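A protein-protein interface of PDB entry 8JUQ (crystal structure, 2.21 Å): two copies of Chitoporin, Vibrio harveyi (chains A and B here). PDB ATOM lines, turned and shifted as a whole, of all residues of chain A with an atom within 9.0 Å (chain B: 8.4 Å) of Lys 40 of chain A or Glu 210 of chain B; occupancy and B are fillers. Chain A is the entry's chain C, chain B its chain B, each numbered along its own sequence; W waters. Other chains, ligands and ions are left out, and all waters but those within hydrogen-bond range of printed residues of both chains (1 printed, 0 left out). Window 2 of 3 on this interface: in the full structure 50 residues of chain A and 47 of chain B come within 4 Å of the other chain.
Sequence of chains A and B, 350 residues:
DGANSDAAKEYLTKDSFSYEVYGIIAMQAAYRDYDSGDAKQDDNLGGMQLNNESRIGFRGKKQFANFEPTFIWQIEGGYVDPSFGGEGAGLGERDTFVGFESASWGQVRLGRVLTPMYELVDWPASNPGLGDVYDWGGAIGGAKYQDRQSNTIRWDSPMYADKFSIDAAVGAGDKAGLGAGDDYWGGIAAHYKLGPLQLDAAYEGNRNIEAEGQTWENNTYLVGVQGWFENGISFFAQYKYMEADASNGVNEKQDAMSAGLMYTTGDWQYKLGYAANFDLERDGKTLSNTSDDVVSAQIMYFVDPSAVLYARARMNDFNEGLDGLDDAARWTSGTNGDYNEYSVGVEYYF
Gly 181 of chain B touches Asp 43 of chain A.
Asp 43 of chain A touches Asp 182 of chain B (O to CB, 3.5 Å).
Ala 180 of chain B touches Asn 44 of chain A (C to CG, 3.6 Å).
N of Leu 45 of chain A touches O of Gly 179 of chain B, 3.6 Å away.
N of Ala 180 of chain B lies within hydrogen-bond range of O of Lys 175 of chain B.
The side-chain amide nitrogen (ND2) of Asn 208 of chain B lies within hydrogen-bond range of the backbone carbonyl oxygen (O) of Asp 182 of chain B (3.2 Å).
NZ of Lys 40 of chain A lies within hydrogen-bond range of OD1 of Asn 44 of chain A.
Water W1 lies within hydrogen-bond range of O of Ala 176 of chain B (2.6 Å) and O of Gly 46 of chain A (3.2 Å).
Of the 23 printed residues of chain B, 5 touch a printed residue of chain A.
Of the 12 printed residues of chain A, 4 touch a printed residue of chain B.
Hydrophobic or aromatic side chains of chain A within 4 Å of the printed part of chain B: Leu 45.
Among the printed residues, 7 pairs touch across the chains.
Among the printed residues, Asp or Glu carboxylates within 4 Å of a Lys or Arg side-chain nitrogen of the other chain: Lys 40 of chain A with Glu 210 of chain B (2.8 Å).
No residue of chain B comes within 4 Å of Ala 39 of chain A.
Of chain B, only Glu 210 (2.8 Å) comes within 4 Å of Lys 40 of chain A.
Of the printed residues of chain B, Asn 44 of chain A touches Gly 179, Ala 180 and Gly 181.
Printed residues of chain A within 4 Å of Gly 179 of chain B: Asn 44 (3.1 Å) and Leu 45 (3.6 Å).
Of the printed residues of chain A, Ala 180 of chain B touches Asn 44.
Printed residues of chain A within 4 Å of Asp 182 of chain B: Asp 43.
Asp 183 of chain B touches none of the printed residues of chain A.
Of chain A, only Lys 40 (2.8 Å) comes within 4 Å of Glu 210 of chain B.
No residue of chain A comes within 4 Å of Ala 211 of chain B.
Glu 212 of chain B touches none of the printed residues of chain A.
The nearest residue of chain A that does not touch Glu 210 of chain B is Asn 44 of chain A (4.9 Å).
The backbone NH of Gly 181 of chain B lies close to the side-chain amide oxygen of Asn 44 of chain A.
The side-chain amino group of Lys 40 of chain A lies within salt-bridge range of the side-chain carboxylate of Glu 210 of chain B (2.8 Å).
O of Asn 44 of chain A lies close to O of Gly 179 of chain B (3.2 Å).
No position is printed for both chains.
Of the 7 pairs that touch across the chains among the printed residues, none has its exchanged pair printed and touching as well.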
ATOM      1  N   TYR A  34      -8.889 -11.909  -8.844  1.00  0.00           N
ATOM      2  CA  TYR A  34      -9.020 -12.537  -7.525  1.00  0.00           C
ATOM      3  C   TYR A  34      -8.717 -14.034  -7.568  1.00  0.00           C
ATOM      4  O   TYR A  34      -9.035 -14.726  -8.535  1.00  0.00           O
ATOM      5  CB  TYR A  34     -10.427 -12.357  -6.929  1.00  0.00           C
ATOM      6  CG  TYR A  34     -10.652 -11.050  -6.182  1.00  0.00           C
ATOM      7  CD1 TYR A  34     -10.858  -9.858  -6.880  1.00  0.00           C
ATOM      8  CD2 TYR A  34     -10.682 -11.008  -4.779  1.00  0.00           C
ATOM      9  CE1 TYR A  34     -11.058  -8.660  -6.214  1.00  0.00           C
ATOM     10  CE2 TYR A  34     -10.900  -9.805  -4.099  1.00  0.00           C
ATOM     11  CZ  TYR A  34     -11.080  -8.633  -4.835  1.00  0.00           C
ATOM     12  OH  TYR A  34     -11.287  -7.425  -4.209  1.00  0.00           O
ATOM     13  N   SER A  36      -9.857 -16.437  -4.818  1.00  0.00           N
ATOM     14  CA  SER A  36     -10.524 -16.650  -3.539  1.00  0.00           C
ATOM     15  C   SER A  36     -10.788 -18.116  -3.244  1.00  0.00           C
ATOM     16  O   SER A  36     -11.184 -18.433  -2.127  1.00  0.00           O
ATOM     17  CB  SER A  36     -11.857 -15.899  -3.494  1.00  0.00           C
ATOM     18  OG  SER A  36     -12.796 -16.541  -4.346  1.00  0.00           O
ATOM     19  N   GLY A  37     -10.611 -19.006  -4.215  1.00  0.00           N
ATOM     20  CA  GLY A  37     -10.954 -20.399  -4.046  1.00  0.00           C
ATOM     21  C   GLY A  37     -12.322 -20.765  -4.559  1.00  0.00           C
ATOM     22  O   GLY A  37     -12.681 -21.945  -4.525  1.00  0.00           O
ATOM     23  N   ASP A  38     -13.087 -19.793  -5.042  1.00  0.00           N
ATOM     24  CA  ASP A  38     -14.402 -20.018  -5.619  1.00  0.00           C
ATOM     25  C   ASP A  38     -14.477 -19.216  -6.909  1.00  0.00           C
ATOM     26  O   ASP A  38     -14.341 -17.990  -6.883  1.00  0.00           O
ATOM     27  CB  ASP A  38     -15.499 -19.591  -4.647  1.00  0.00           C
ATOM     28  CG  ASP A  38     -16.873 -19.817  -5.206  1.00  0.00           C
ATOM     29  OD1 ASP A  38     -17.625 -18.836  -5.373  1.00  0.00           O
ATOM     30  OD2 ASP A  38     -17.199 -20.997  -5.494  1.00  0.00           O
ATOM     31  N   ALA A  39     -14.691 -19.899  -8.035  1.00  0.00           N
ATOM     32  CA  ALA A  39     -14.604 -19.232  -9.328  1.00  0.00           C
ATOM     33  C   ALA A  39     -15.684 -18.170  -9.484  1.00  0.00           C
ATOM     34  O   ALA A  39     -15.443 -17.121 -10.104  1.00  0.00           O
ATOM     35  CB  ALA A  39     -14.698 -20.242 -10.468  1.00  0.00           C
ATOM     36  N   LYS A  40     -16.881 -18.430  -8.951  1.00  0.00           N
ATOM     37  CA  LYS A  40     -17.966 -17.460  -9.082  1.00  0.00           C
ATOM     38  C   LYS A  40     -17.643 -16.178  -8.323  1.00  0.00           C
ATOM     39  O   LYS A  40     -17.828 -15.074  -8.846  1.00  0.00           O
ATOM     40  CB  LYS A  40     -19.276 -18.068  -8.582  1.00  0.00           C
ATOM     41  CG  LYS A  40     -20.515 -17.165  -8.737  1.00  0.00           C
ATOM     42  CD  LYS A  40     -20.799 -16.794 -10.200  1.00  0.00           C
ATOM     43  CE  LYS A  40     -21.828 -15.641 -10.328  1.00  0.00           C
ATOM     44  NZ  LYS A  40     -21.717 -14.903 -11.647  1.00  0.00           N
ATOM     45  N   GLN A  41     -17.152 -16.317  -7.089  1.00  0.00           N
ATOM     46  CA  GLN A  41     -16.724 -15.172  -6.294  1.00  0.00           C
ATOM     47  C   GLN A  41     -15.584 -14.415  -6.982  1.00  0.00           C
ATOM     48  O   GLN A  41     -15.574 -13.177  -6.996  1.00  0.00           O
ATOM     49  CB  GLN A  41     -16.325 -15.667  -4.898  1.00  0.00           C
ATOM     50  CG  GLN A  41     -16.346 -14.608  -3.790  1.00  0.00           C
ATOM     51  CD  GLN A  41     -15.376 -14.953  -2.657  1.00  0.00           C
ATOM     52  OE1 GLN A  41     -14.692 -14.085  -2.105  1.00  0.00           O
ATOM     53  NE2 GLN A  41     -15.322 -16.236  -2.304  1.00  0.00           N
ATOM     54  N   ASP A  42     -14.636 -15.142  -7.589  1.00  0.00           N
ATOM     55  CA  ASP A  42     -13.558 -14.499  -8.337  1.00  0.00           C
ATOM     56  C   ASP A  42     -14.115 -13.668  -9.489  1.00  0.00           C
ATOM     57  O   ASP A  42     -13.674 -12.531  -9.714  1.00  0.00           O
ATOM     58  CB  ASP A  42     -12.587 -15.550  -8.888  1.00  0.00           C
ATOM     59  CG  ASP A  42     -11.696 -16.182  -7.810  1.00  0.00           C
ATOM     60  OD1 ASP A  42     -11.678 -15.681  -6.659  1.00  0.00           O
ATOM     61  OD2 ASP A  42     -11.041 -17.214  -8.109  1.00  0.00           O
ATOM     62  N   ASP A  43     -15.134 -14.197 -10.188  1.00  0.00           N
ATOM     63  CA  ASP A  43     -15.715 -13.493 -11.332  1.00  0.00           C
ATOM     64  C   ASP A  43     -16.471 -12.238 -10.897  1.00  0.00           C
ATOM     65  O   ASP A  43     -16.383 -11.201 -11.560  1.00  0.00           O
ATOM     66  CB  ASP A  43     -16.671 -14.412 -12.103  1.00  0.00           C
ATOM     67  CG  ASP A  43     -15.967 -15.606 -12.772  1.00  0.00           C
ATOM     68  OD1 ASP A  43     -14.743 -15.542 -13.055  1.00  0.00           O
ATOM     69  OD2 ASP A  43     -16.656 -16.628 -13.003  1.00  0.00           O
ATOM     70  N   ASN A  44     -17.224 -12.329  -9.793  1.00  0.00           N
ATOM     71  CA  ASN A  44     -18.020 -11.215  -9.276  1.00  0.00           C
ATOM     72  C   ASN A  44     -17.145 -10.061  -8.790  1.00  0.00           C
ATOM     73  O   ASN A  44     -17.402  -8.896  -9.119  1.00  0.00           O
ATOM     74  CB  ASN A  44     -18.909 -11.722  -8.145  1.00  0.00           C
ATOM     75  CG  ASN A  44     -20.047 -12.593  -8.649  1.00  0.00           C
ATOM     76  OD1 ASN A  44     -20.321 -12.671  -9.859  1.00  0.00           O
ATOM     77  ND2 ASN A  44     -20.743 -13.212  -7.728  1.00  0.00           N
ATOM     78  N   LEU A  45     -16.153 -10.367  -7.946  1.00  0.00           N
ATOM     79  CA  LEU A  45     -15.296  -9.359  -7.333  1.00  0.00           C
ATOM     80  C   LEU A  45     -14.275  -8.823  -8.315  1.00  0.00           C
ATOM     81  O   LEU A  45     -13.903  -7.650  -8.248  1.00  0.00           O
ATOM     82  CB  LEU A  45     -14.574  -9.933  -6.116  1.00  0.00           C
ATOM     83  CG  LEU A  45     -15.430 -10.282  -4.899  1.00  0.00           C
ATOM     84  CD1 LEU A  45     -14.624 -11.162  -3.928  1.00  0.00           C
ATOM     85  CD2 LEU A  45     -15.896  -9.028  -4.220  1.00  0.00           C
ATOM     86  N   GLY A  46     -13.771  -9.673  -9.199  1.00  0.00           N
ATOM     87  CA  GLY A  46     -12.721  -9.274 -10.110  1.00  0.00           C
ATOM     88  C   GLY A  46     -13.264  -8.660 -11.379  1.00  0.00           C
ATOM     89  O   GLY A  46     -14.464  -8.582 -11.622  1.00  0.00           O
ATOM     90  N   GLY B 142     -33.590  -9.737 -19.229  1.00  0.00           N
ATOM     91  CA  GLY B 142     -32.199  -9.309 -19.272  1.00  0.00           C
ATOM     92  C   GLY B 142     -32.127  -7.794 -19.175  1.00  0.00           C
ATOM     93  O   GLY B 142     -32.848  -7.167 -18.402  1.00  0.00           O
ATOM     94  N   ALA B 143     -31.248  -7.188 -19.966  1.00  0.00           N
ATOM     95  CA  ALA B 143     -31.109  -5.731 -19.997  1.00  0.00           C
ATOM     96  C   ALA B 143     -31.038  -5.280 -21.449  1.00  0.00           C
ATOM     97  O   ALA B 143     -30.019  -5.502 -22.112  1.00  0.00           O
ATOM     98  CB  ALA B 143     -29.863  -5.302 -19.231  1.00  0.00           C
ATOM     99  N   LYS B 175     -24.210  -5.105 -11.734  1.00  0.00           N
ATOM    100  CA  LYS B 175     -23.732  -5.918 -10.616  1.00  0.00           C
ATOM    101  C   LYS B 175     -22.215  -5.891 -10.526  1.00  0.00           C
ATOM    102  O   LYS B 175     -21.650  -5.859  -9.419  1.00  0.00           O
ATOM    103  CB  LYS B 175     -24.237  -7.356 -10.751  1.00  0.00           C
ATOM    104  CG  LYS B 175     -25.742  -7.448 -10.568  1.00  0.00           C
ATOM    105  CD  LYS B 175     -26.196  -8.902 -10.492  1.00  0.00           C
ATOM    106  CE  LYS B 175     -27.710  -8.974 -10.380  1.00  0.00           C
ATOM    107  NZ  LYS B 175     -28.108  -8.205  -9.161  1.00  0.00           N
ATOM    108  N   ALA B 176     -21.540  -5.921 -11.681  1.00  0.00           N
ATOM    109  CA  ALA B 176     -20.089  -5.844 -11.711  1.00  0.00           C
ATOM    110  C   ALA B 176     -19.580  -4.574 -11.048  1.00  0.00           C
ATOM    111  O   ALA B 176     -18.491  -4.581 -10.466  1.00  0.00           O
ATOM    112  CB  ALA B 176     -19.580  -5.918 -13.159  1.00  0.00           C
ATOM    113  N   GLY B 179     -19.041  -5.338  -7.525  1.00  0.00           N
ATOM    114  CA  GLY B 179     -18.352  -6.570  -7.204  1.00  0.00           C
ATOM    115  C   GLY B 179     -19.270  -7.765  -6.977  1.00  0.00           C
ATOM    116  O   GLY B 179     -18.864  -8.721  -6.329  1.00  0.00           O
ATOM    117  N   ALA B 180     -20.479  -7.745  -7.546  1.00  0.00           N
ATOM    118  CA  ALA B 180     -21.499  -8.763  -7.337  1.00  0.00           C
ATOM    119  C   ALA B 180     -21.880  -9.484  -8.635  1.00  0.00           C
ATOM    120  O   ALA B 180     -22.903 -10.169  -8.658  1.00  0.00           O
ATOM    121  CB  ALA B 180     -22.758  -8.144  -6.709  1.00  0.00           C
ATOM    122  N   GLY B 181     -21.097  -9.345  -9.705  1.00  0.00           N
ATOM    123  CA  GLY B 181     -21.419  -9.988 -10.969  1.00  0.00           C
ATOM    124  C   GLY B 181     -20.308  -9.738 -11.971  1.00  0.00           C
ATOM    125  O   GLY B 181     -19.355  -9.000 -11.712  1.00  0.00           O
ATOM    126  N   ASP B 182     -20.442 -10.341 -13.141  1.00  0.00           N
ATOM    127  CA  ASP B 182     -19.466 -10.085 -14.192  1.00  0.00           C
ATOM    128  C   ASP B 182     -20.158  -9.700 -15.498  1.00  0.00           C
ATOM    129  O   ASP B 182     -19.675  -9.998 -16.595  1.00  0.00           O
ATOM    130  CB  ASP B 182     -18.525 -11.274 -14.349  1.00  0.00           C
ATOM    131  CG  ASP B 182     -19.241 -12.528 -14.813  1.00  0.00           C
ATOM    132  OD1 ASP B 182     -20.483 -12.556 -14.725  1.00  0.00           O
ATOM    133  OD2 ASP B 182     -18.563 -13.464 -15.292  1.00  0.00           O
ATOM    134  N   ASP B 183     -21.289  -9.014 -15.378  1.00  0.00           N
ATOM    135  CA  ASP B 183     -21.977  -8.449 -16.526  1.00  0.00           C
ATOM    136  C   ASP B 183     -21.154  -7.317 -17.160  1.00  0.00           C
ATOM    137  O   ASP B 183     -20.295  -6.696 -16.529  1.00  0.00           O
ATOM    138  CB  ASP B 183     -23.408  -8.024 -16.107  1.00  0.00           C
ATOM    139  CG  ASP B 183     -23.446  -7.162 -14.822  1.00  0.00           C
ATOM    140  OD1 ASP B 183     -22.439  -7.170 -14.063  1.00  0.00           O
ATOM    141  OD2 ASP B 183     -24.533  -6.574 -14.502  1.00  0.00           O
ATOM    142  N   TYR B 184     -21.345  -7.130 -18.453  1.00  0.00           N
ATOM    143  CA  TYR B 184     -20.672  -6.079 -19.194  1.00  0.00           C
ATOM    144  C   TYR B 184     -21.477  -5.835 -20.467  1.00  0.00           C
ATOM    145  O   TYR B 184     -22.434  -6.550 -20.769  1.00  0.00           O
ATOM    146  CB  TYR B 184     -19.203  -6.436 -19.496  1.00  0.00           C
ATOM    147  CG  TYR B 184     -19.045  -7.605 -20.444  1.00  0.00           C
ATOM    148  CD1 TYR B 184     -19.059  -8.918 -19.970  1.00  0.00           C
ATOM    149  CD2 TYR B 184     -18.874  -7.401 -21.812  1.00  0.00           C
ATOM    150  CE1 TYR B 184     -18.910  -9.986 -20.831  1.00  0.00           C
ATOM    151  CE2 TYR B 184     -18.720  -8.469 -22.687  1.00  0.00           C
ATOM    152  CZ  TYR B 184     -18.737  -9.751 -22.188  1.00  0.00           C
ATOM    153  OH  TYR B 184     -18.599 -10.808 -23.046  1.00  0.00           O
ATOM    154  N   ARG B 207     -24.062  -8.531 -21.788  1.00  0.00           N
ATOM    155  CA  ARG B 207     -23.604  -9.901 -21.590  1.00  0.00           C
ATOM    156  C   ARG B 207     -23.535 -10.250 -20.105  1.00  0.00           C
ATOM    157  O   ARG B 207     -23.285  -9.388 -19.252  1.00  0.00           O
ATOM    158  CB  ARG B 207     -22.228 -10.103 -22.236  1.00  0.00           C
ATOM    159  CG  ARG B 207     -22.181  -9.781 -23.744  1.00  0.00           C
ATOM    160  CD  ARG B 207     -23.002 -10.799 -24.543  1.00  0.00           C
ATOM    161  NE  ARG B 207     -22.875 -10.625 -25.988  1.00  0.00           N
ATOM    162  CZ  ARG B 207     -23.766 -10.007 -26.762  1.00  0.00           C
ATOM    163  NH1 ARG B 207     -24.878  -9.467 -26.260  1.00  0.00           N
ATOM    164  NH2 ARG B 207     -23.523  -9.900 -28.061  1.00  0.00           N
ATOM    165  N   ASN B 208     -23.770 -11.532 -19.805  1.00  0.00           N
ATOM    166  CA  ASN B 208     -23.655 -12.067 -18.440  1.00  0.00           C
ATOM    167  C   ASN B 208     -24.622 -11.401 -17.477  1.00  0.00           C
ATOM    168  O   ASN B 208     -24.289 -11.185 -16.307  1.00  0.00           O
ATOM    169  CB  ASN B 208     -22.233 -11.939 -17.879  1.00  0.00           C
ATOM    170  CG  ASN B 208     -21.254 -12.802 -18.609  1.00  0.00           C
ATOM    171  OD1 ASN B 208     -21.652 -13.649 -19.397  1.00  0.00           O
ATOM    172  ND2 ASN B 208     -19.960 -12.595 -18.366  1.00  0.00           N
ATOM    173  N   ILE B 209     -25.804 -11.041 -17.955  1.00  0.00           N
ATOM    174  CA  ILE B 209     -26.822 -10.445 -17.101  1.00  0.00           C
ATOM    175  C   ILE B 209     -27.539 -11.533 -16.303  1.00  0.00           C
ATOM    176  O   ILE B 209     -28.068 -12.499 -16.871  1.00  0.00           O
ATOM    177  CB  ILE B 209     -27.809  -9.635 -17.942  1.00  0.00           C
ATOM    178  CG1 ILE B 209     -27.015  -8.652 -18.827  1.00  0.00           C
ATOM    179  CG2 ILE B 209     -28.864  -8.963 -17.031  1.00  0.00           C
ATOM    180  CD1 ILE B 209     -26.854  -7.248 -18.224  1.00  0.00           C
ATOM    181  N   GLU B 210     -27.565 -11.373 -14.983  1.00  0.00           N
ATOM    182  CA  GLU B 210     -28.198 -12.321 -14.075  1.00  0.00           C
ATOM    183  C   GLU B 210     -29.566 -11.784 -13.705  1.00  0.00           C
ATOM    184  O   GLU B 210     -29.665 -10.691 -13.145  1.00  0.00           O
ATOM    185  CB  GLU B 210     -27.345 -12.518 -12.821  1.00  0.00           C
ATOM    186  CG  GLU B 210     -26.131 -13.438 -13.016  1.00  0.00           C
ATOM    187  CD  GLU B 210     -25.228 -13.504 -11.772  1.00  0.00           C
ATOM    188  OE1 GLU B 210     -25.238 -12.536 -10.962  1.00  0.00           O
ATOM    189  OE2 GLU B 210     -24.507 -14.520 -11.603  1.00  0.00           O
ATOM    190  N   ALA B 211     -30.613 -12.543 -14.024  1.00  0.00           N
ATOM    191  CA  ALA B 211     -31.984 -12.154 -13.723  1.00  0.00           C
ATOM    192  C   ALA B 211     -32.899 -13.370 -13.840  1.00  0.00           C
ATOM    193  O   ALA B 211     -32.702 -14.215 -14.722  1.00  0.00           O
ATOM    194  CB  ALA B 211     -32.477 -11.050 -14.660  1.00  0.00           C
ATOM    195  N   GLU B 212     -33.878 -13.462 -12.929  1.00  0.00           N
ATOM    196  CA  GLU B 212     -34.927 -14.491 -12.991  1.00  0.00           C
ATOM    197  C   GLU B 212     -34.347 -15.906 -13.024  1.00  0.00           C
ATOM    198  O   GLU B 212     -34.863 -16.784 -13.723  1.00  0.00           O
ATOM    199  CB  GLU B 212     -35.840 -14.265 -14.202  1.00  0.00           C
ATOM    200  CG  GLU B 212     -36.359 -12.850 -14.314  1.00  0.00           C
ATOM    201  CD  GLU B 212     -37.058 -12.590 -15.629  1.00  0.00           C
ATOM    202  OE1 GLU B 212     -37.047 -13.503 -16.482  1.00  0.00           O
ATOM    203  OE2 GLU B 212     -37.630 -11.480 -15.801  1.00  0.00           O
ATOM    204  N   GLY B 213     -33.243 -16.114 -12.297  1.00  0.00           N
ATOM    205  CA  GLY B 213     -32.556 -17.390 -12.225  1.00  0.00           C
ATOM    206  C   GLY B 213     -31.758 -17.801 -13.447  1.00  0.00           C
ATOM    207  O   GLY B 213     -31.216 -18.908 -13.465  1.00  0.00           O
ATOM    208  N   GLN B 214     -31.628 -16.945 -14.452  1.00  0.00           N
ATOM    209  CA  GLN B 214     -30.888 -17.270 -15.663  1.00  0.00           C
ATOM    210  C   GLN B 214     -29.772 -16.253 -15.900  1.00  0.00           C
ATOM    211  O   GLN B 214     -29.718 -15.197 -15.259  1.00  0.00           O
ATOM    212  CB  GLN B 214     -31.827 -17.300 -16.874  1.00  0.00           C
ATOM    213  CG  GLN B 214     -33.038 -18.206 -16.706  1.00  0.00           C
ATOM    214  CD  GLN B 214     -32.634 -19.656 -16.550  1.00  0.00           C
ATOM    215  OE1 GLN B 214     -31.748 -20.154 -17.260  1.00  0.00           O
ATOM    216  NE2 GLN B 214     -33.264 -20.341 -15.604  1.00  0.00           N
ATOM    217  N   THR B 215     -28.891 -16.580 -16.850  1.00  0.00           N
ATOM    218  CA  THR B 215     -27.914 -15.644 -17.409  1.00  0.00           C
ATOM    219  C   THR B 215     -28.385 -15.222 -18.804  1.00  0.00           C
ATOM    220  O   THR B 215     -28.797 -16.065 -19.608  1.00  0.00           O
ATOM    221  CB  THR B 215     -26.519 -16.279 -17.474  1.00  0.00           C
ATOM    222  OG1 THR B 215     -26.091 -16.650 -16.155  1.00  0.00           O
ATOM    223  CG2 THR B 215     -25.489 -15.302 -18.042  1.00  0.00           C
ATOM    224  N   TRP B 216     -28.327 -13.924 -19.093  1.00  0.00           N
ATOM    225  CA  TRP B 216     -28.922 -13.396 -20.310  1.00  0.00           C
ATOM    226  C   TRP B 216     -27.884 -12.727 -21.198  1.00  0.00           C
ATOM    227  O   TRP B 216     -26.917 -12.137 -20.712  1.00  0.00           O
ATOM    228  CB  TRP B 216     -30.007 -12.365 -20.007  1.00  0.00           C
ATOM    229  CG  TRP B 216     -31.229 -12.868 -19.311  1.00  0.00           C
ATOM    230  CD1 TRP B 216     -31.354 -13.128 -17.984  1.00  0.00           C
ATOM    231  CD2 TRP B 216     -32.514 -13.124 -19.897  1.00  0.00           C
ATOM    232  NE1 TRP B 216     -32.634 -13.525 -17.704  1.00  0.00           N
ATOM    233  CE2 TRP B 216     -33.369 -13.532 -18.859  1.00  0.00           C
ATOM    234  CE3 TRP B 216     -33.018 -13.059 -21.204  1.00  0.00           C
ATOM    235  CZ2 TRP B 216     -34.714 -13.884 -19.079  1.00  0.00           C
ATOM    236  CZ3 TRP B 216     -34.362 -13.399 -21.429  1.00  0.00           C
ATOM    237  CH2 TRP B 216     -35.192 -13.810 -20.366  1.00  0.00           C
ATOM    238  N   GLU B 217     -28.115 -12.799 -22.507  1.00  0.00           N
ATOM    239  CA  GLU B 217     -27.460 -11.930 -23.478  1.00  0.00           C
ATOM    240  C   GLU B 217     -28.516 -11.083 -24.175  1.00  0.00           C
ATOM    241  O   GLU B 217     -29.574 -11.578 -24.547  1.00  0.00           O
ATOM    242  CB  GLU B 217     -26.656 -12.736 -24.503  1.00  0.00           C
ATOM    243  CG  GLU B 217     -25.726 -13.702 -23.795  1.00  0.00           C
ATOM    244  CD  GLU B 217     -24.519 -14.108 -24.620  1.00  0.00           C
ATOM    245  OE1 GLU B 217     -24.527 -13.847 -25.846  1.00  0.00           O
ATOM    246  OE2 GLU B 217     -23.549 -14.659 -24.026  1.00  0.00           O
ATOM    247  N   ASN B 218     -28.241  -9.807 -24.346  1.00  0.00           N
ATOM    248  CA  ASN B 218     -29.169  -8.937 -25.037  1.00  0.00           C
ATOM    249  C   ASN B 218     -28.463  -8.328 -26.233  1.00  0.00           C
ATOM    250  O   ASN B 218     -27.261  -8.043 -26.177  1.00  0.00           O
ATOM    251  CB  ASN B 218     -29.674  -7.825 -24.130  1.00  0.00           C
ATOM    252  CG  ASN B 218     -30.611  -8.334 -23.038  1.00  0.00           C
ATOM    253  OD1 ASN B 218     -30.168  -8.914 -22.046  1.00  0.00           O
ATOM    254  ND2 ASN B 218     -31.904  -8.086 -23.205  1.00  0.00           N
ATOM    255  N   SER B 247     -29.941 -18.476 -20.678  1.00  0.00           N
ATOM    256  CA  SER B 247     -29.048 -19.636 -20.645  1.00  0.00           C
ATOM    257  C   SER B 247     -29.785 -20.979 -20.651  1.00  0.00           C
ATOM    258  O   SER B 247     -29.130 -22.013 -20.784  1.00  0.00           O
ATOM    259  CB  SER B 247     -28.110 -19.574 -19.427  1.00  0.00           C
ATOM    260  OG  SER B 247     -28.777 -19.220 -18.203  1.00  0.00           O
HETATM  261  O   HOH W   1     -16.558  -6.214 -11.243  1.00  0.00           O
